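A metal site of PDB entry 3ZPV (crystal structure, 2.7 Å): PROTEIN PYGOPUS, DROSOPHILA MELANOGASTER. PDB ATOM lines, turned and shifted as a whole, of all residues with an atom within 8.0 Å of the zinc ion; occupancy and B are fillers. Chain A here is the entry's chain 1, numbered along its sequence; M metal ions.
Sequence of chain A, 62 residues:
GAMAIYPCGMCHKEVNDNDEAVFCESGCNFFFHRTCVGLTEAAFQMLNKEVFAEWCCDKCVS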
ATOM      1  N   PHE A  23      21.981   0.182 -21.106  1.00  0.00           N
ATOM      2  CA  PHE A  23      21.002   0.111 -22.178  1.00  0.00           C
ATOM      3  C   PHE A  23      19.600   0.318 -21.638  1.00  0.00           C
ATOM      4  O   PHE A  23      19.250  -0.281 -20.641  1.00  0.00           O
ATOM      5  CB  PHE A  23      21.063  -1.256 -22.819  1.00  0.00           C
ATOM      6  CG  PHE A  23      20.110  -1.429 -23.942  1.00  0.00           C
ATOM      7  CD1 PHE A  23      20.359  -0.847 -25.168  1.00  0.00           C
ATOM      8  CD2 PHE A  23      18.974  -2.162 -23.781  1.00  0.00           C
ATOM      9  CE1 PHE A  23      19.462  -0.981 -26.223  1.00  0.00           C
ATOM     10  CE2 PHE A  23      18.064  -2.297 -24.817  1.00  0.00           C
ATOM     11  CZ  PHE A  23      18.320  -1.710 -26.055  1.00  0.00           C
ATOM     12  N   CYS A  24      18.825   1.214 -22.238  1.00  0.00           N
ATOM     13  CA  CYS A  24      17.509   1.522 -21.709  1.00  0.00           C
ATOM     14  C   CYS A  24      16.573   0.473 -22.254  1.00  0.00           C
ATOM     15  O   CYS A  24      16.305   0.419 -23.449  1.00  0.00           O
ATOM     16  CB  CYS A  24      17.054   2.934 -22.099  1.00  0.00           C
ATOM     17  SG  CYS A  24      15.406   3.379 -21.456  1.00  0.00           S
ATOM     18  N   GLU A  25      16.053  -0.345 -21.363  1.00  0.00           N
ATOM     19  CA  GLU A  25      15.117  -1.415 -21.740  1.00  0.00           C
ATOM     20  C   GLU A  25      13.635  -0.986 -21.642  1.00  0.00           C
ATOM     21  O   GLU A  25      12.746  -1.739 -21.998  1.00  0.00           O
ATOM     22  CB  GLU A  25      15.413  -2.698 -20.932  1.00  0.00           C
ATOM     23  CG  GLU A  25      16.461  -3.739 -21.508  1.00  0.00           C
ATOM     24  CD  GLU A  25      15.944  -4.586 -22.647  1.00  0.00           C
ATOM     25  OE1 GLU A  25      15.061  -5.447 -22.416  1.00  0.00           O
ATOM     26  OE2 GLU A  25      16.472  -4.431 -23.774  1.00  0.00           O
ATOM     27  N   SER A  26      13.348   0.258 -21.249  1.00  0.00           N
ATOM     28  CA  SER A  26      11.964   0.717 -21.085  1.00  0.00           C
ATOM     29  C   SER A  26      11.370   1.386 -22.314  1.00  0.00           C
ATOM     30  O   SER A  26      10.273   1.922 -22.208  1.00  0.00           O
ATOM     31  CB  SER A  26      11.844   1.680 -19.892  1.00  0.00           C
ATOM     32  OG  SER A  26      12.111   1.009 -18.681  1.00  0.00           O
ATOM     33  N   GLY A  27      12.054   1.424 -23.445  1.00  0.00           N
ATOM     34  CA  GLY A  27      11.400   1.933 -24.637  1.00  0.00           C
ATOM     35  C   GLY A  27      12.205   2.621 -25.698  1.00  0.00           C
ATOM     36  O   GLY A  27      11.999   2.340 -26.887  1.00  0.00           O
ATOM     37  N   CYS A  28      13.096   3.546 -25.321  1.00  0.00           N
ATOM     38  CA  CYS A  28      13.876   4.267 -26.337  1.00  0.00           C
ATOM     39  C   CYS A  28      14.876   3.377 -27.106  1.00  0.00           C
ATOM     40  O   CYS A  28      15.266   3.692 -28.225  1.00  0.00           O
ATOM     41  CB  CYS A  28      14.568   5.490 -25.767  1.00  0.00           C
ATOM     42  SG  CYS A  28      15.889   5.224 -24.591  1.00  0.00           S
ATOM     43  N   ASN A  29      15.281   2.267 -26.500  1.00  0.00           N
ATOM     44  CA  ASN A  29      16.242   1.337 -27.111  1.00  0.00           C
ATOM     45  C   ASN A  29      17.617   1.925 -27.446  1.00  0.00           C
ATOM     46  O   ASN A  29      18.270   1.466 -28.358  1.00  0.00           O
ATOM     47  CB  ASN A  29      15.630   0.703 -28.360  1.00  0.00           C
ATOM     48  CG  ASN A  29      14.589  -0.332 -28.011  1.00  0.00           C
ATOM     49  OD1 ASN A  29      14.499  -0.788 -26.862  1.00  0.00           O
ATOM     50  ND2 ASN A  29      13.840  -0.751 -28.998  1.00  0.00           N
ATOM     51  N   PHE A  30      18.027   2.946 -26.689  1.00  0.00           N
ATOM     52  CA  PHE A  30      19.341   3.529 -26.845  1.00  0.00           C
ATOM     53  C   PHE A  30      20.347   2.932 -25.850  1.00  0.00           C
ATOM     54  O   PHE A  30      20.010   2.677 -24.693  1.00  0.00           O
ATOM     55  CB  PHE A  30      19.277   5.022 -26.601  1.00  0.00           C
ATOM     56  CG  PHE A  30      18.998   5.818 -27.834  1.00  0.00           C
ATOM     57  CD1 PHE A  30      20.030   6.141 -28.719  1.00  0.00           C
ATOM     58  CD2 PHE A  30      17.725   6.290 -28.080  1.00  0.00           C
ATOM     59  CE1 PHE A  30      19.777   6.914 -29.832  1.00  0.00           C
ATOM     60  CE2 PHE A  30      17.466   7.067 -29.186  1.00  0.00           C
ATOM     61  CZ  PHE A  30      18.500   7.368 -30.071  1.00  0.00           C
ATOM     62  N   PHE A  32      23.784   4.011 -23.832  1.00  0.00           N
ATOM     63  CA  PHE A  32      24.305   5.246 -23.255  1.00  0.00           C
ATOM     64  C   PHE A  32      25.629   4.958 -22.575  1.00  0.00           C
ATOM     65  O   PHE A  32      25.798   3.929 -21.955  1.00  0.00           O
ATOM     66  CB  PHE A  32      23.380   5.760 -22.162  1.00  0.00           C
ATOM     67  CG  PHE A  32      22.000   6.142 -22.603  1.00  0.00           C
ATOM     68  CD1 PHE A  32      21.025   5.187 -22.764  1.00  0.00           C
ATOM     69  CD2 PHE A  32      21.666   7.475 -22.806  1.00  0.00           C
ATOM     70  CE1 PHE A  32      19.747   5.550 -23.152  1.00  0.00           C
ATOM     71  CE2 PHE A  32      20.379   7.864 -23.187  1.00  0.00           C
ATOM     72  CZ  PHE A  32      19.417   6.906 -23.350  1.00  0.00           C
ATOM     73  N   TRP A  55      18.088  -0.818 -15.752  1.00  0.00           N
ATOM     74  CA  TRP A  55      18.188   0.630 -15.798  1.00  0.00           C
ATOM     75  C   TRP A  55      17.214   1.248 -16.806  1.00  0.00           C
ATOM     76  O   TRP A  55      16.819   0.609 -17.774  1.00  0.00           O
ATOM     77  CB  TRP A  55      19.642   1.038 -16.109  1.00  0.00           C
ATOM     78  CG  TRP A  55      19.855   2.493 -16.220  1.00  0.00           C
ATOM     79  CD1 TRP A  55      19.988   3.376 -15.196  1.00  0.00           C
ATOM     80  CD2 TRP A  55      19.891   3.262 -17.430  1.00  0.00           C
ATOM     81  NE1 TRP A  55      20.141   4.655 -15.698  1.00  0.00           N
ATOM     82  CE2 TRP A  55      20.066   4.608 -17.062  1.00  0.00           C
ATOM     83  CE3 TRP A  55      19.800   2.934 -18.795  1.00  0.00           C
ATOM     84  CZ2 TRP A  55      20.174   5.617 -17.990  1.00  0.00           C
ATOM     85  CZ3 TRP A  55      19.873   3.944 -19.711  1.00  0.00           C
ATOM     86  CH2 TRP A  55      20.076   5.276 -19.311  1.00  0.00           C
ATOM     87  N   CYS A  56      16.871   2.525 -16.577  1.00  0.00           N
ATOM     88  CA  CYS A  56      15.946   3.275 -17.420  1.00  0.00           C
ATOM     89  C   CYS A  56      16.399   4.745 -17.551  1.00  0.00           C
ATOM     90  O   CYS A  56      16.819   5.355 -16.560  1.00  0.00           O
ATOM     91  CB  CYS A  56      14.573   3.203 -16.773  1.00  0.00           C
ATOM     92  SG  CYS A  56      13.288   4.070 -17.711  1.00  0.00           S
ATOM     93  N   CYS A  57      16.339   5.300 -18.766  1.00  0.00           N
ATOM     94  CA  CYS A  57      16.770   6.694 -18.987  1.00  0.00           C
ATOM     95  C   CYS A  57      15.731   7.650 -18.427  1.00  0.00           C
ATOM     96  O   CYS A  57      14.628   7.228 -18.127  1.00  0.00           O
ATOM     97  CB  CYS A  57      17.025   6.990 -20.490  1.00  0.00           C
ATOM     98  SG  CYS A  57      15.563   7.133 -21.545  1.00  0.00           S
ATOM     99  N   ASP A  58      16.081   8.920 -18.309  1.00  0.00           N
ATOM    100  CA  ASP A  58      15.175   9.910 -17.713  1.00  0.00           C
ATOM    101  C   ASP A  58      13.929  10.134 -18.549  1.00  0.00           C
ATOM    102  O   ASP A  58      12.843  10.287 -17.999  1.00  0.00           O
ATOM    103  CB  ASP A  58      15.905  11.230 -17.405  1.00  0.00           C
ATOM    104  CG  ASP A  58      16.824  11.112 -16.207  1.00  0.00           C
ATOM    105  OD1 ASP A  58      16.626  10.213 -15.344  1.00  0.00           O
ATOM    106  OD2 ASP A  58      17.817  11.875 -16.137  1.00  0.00           O
ATOM    107  N   LYS A  59      14.092  10.205 -19.864  1.00  0.00           N
ATOM    108  CA  LYS A  59      12.947  10.390 -20.778  1.00  0.00           C
ATOM    109  C   LYS A  59      11.927   9.269 -20.689  1.00  0.00           C
ATOM    110  O   LYS A  59      10.726   9.517 -20.780  1.00  0.00           O
ATOM    111  CB  LYS A  59      13.423  10.546 -22.232  1.00  0.00           C
ATOM    112  CG  LYS A  59      13.921  11.947 -22.542  1.00  0.00           C
ATOM    113  CD  LYS A  59      14.854  11.982 -23.732  1.00  0.00           C
ATOM    114  CE  LYS A  59      15.723  13.239 -23.711  1.00  0.00           C
ATOM    115  NZ  LYS A  59      16.700  13.316 -24.832  1.00  0.00           N
ATOM    116  N   CYS A  60      12.381   8.044 -20.543  1.00  0.00           N
ATOM    117  CA  CYS A  60      11.458   6.929 -20.533  1.00  0.00           C
ATOM    118  C   CYS A  60      10.745   6.718 -19.189  1.00  0.00           C
ATOM    119  O   CYS A  60       9.726   6.034 -19.155  1.00  0.00           O
ATOM    120  CB  CYS A  60      12.180   5.623 -20.938  1.00  0.00           C
ATOM    121  SG  CYS A  60      12.677   5.567 -22.668  1.00  0.00           S
ATOM    122  N   VAL A  61      11.278   7.279 -18.107  1.00  0.00           N
ATOM    123  CA  VAL A  61      10.655   7.128 -16.792  1.00  0.00           C
ATOM    124  C   VAL A  61       9.175   7.551 -16.844  1.00  0.00           C
ATOM    125  O   VAL A  61       8.293   6.832 -16.338  1.00  0.00           O
ATOM    126  CB  VAL A  61      11.407   7.934 -15.704  1.00  0.00           C
ATOM    127  CG1 VAL A  61      10.627   7.932 -14.389  1.00  0.00           C
ATOM    128  CG2 VAL A  61      12.796   7.367 -15.478  1.00  0.00           C
HETATM  129 ZN    ZN M   1      14.862   5.298 -22.536  1.00  0.00          ZN
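The backbone carbonyl oxygen (O) of Phe 30 is in hydrogen-bond range of the backbone NH (N) of Cys 24, 3.1 Å away. SG of Cys 24 sits close to N of Ser 26 (3.7 Å). SG of Cys 28 sits close to N of Phe 30 (3.8 Å). SG of Cys 57 lies close to N of Lys 59 (3.8 Å).
Within 4 Å of the zinc ion: Cys 24, Cys 28, Cys 57 and Cys 60. The nearest printed residue that does not touch the zinc ion is Gly 27 (4.9 Å).
The zinc ion is bound by the side-chain sulfur (SG) of Cys 57 (2.2 Å). The zinc ion is bound by the side-chain sulfur (SG) of Cys 60, 2.2 Å away. The side-chain sulfur (SG) of Cys 24 is bound to the zinc ion (2.3 Å). The side-chain sulfur (SG) of Cys 28 is bound to the zinc ion (2.3 Å). The zinc ion has four donor atoms within binding distance.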
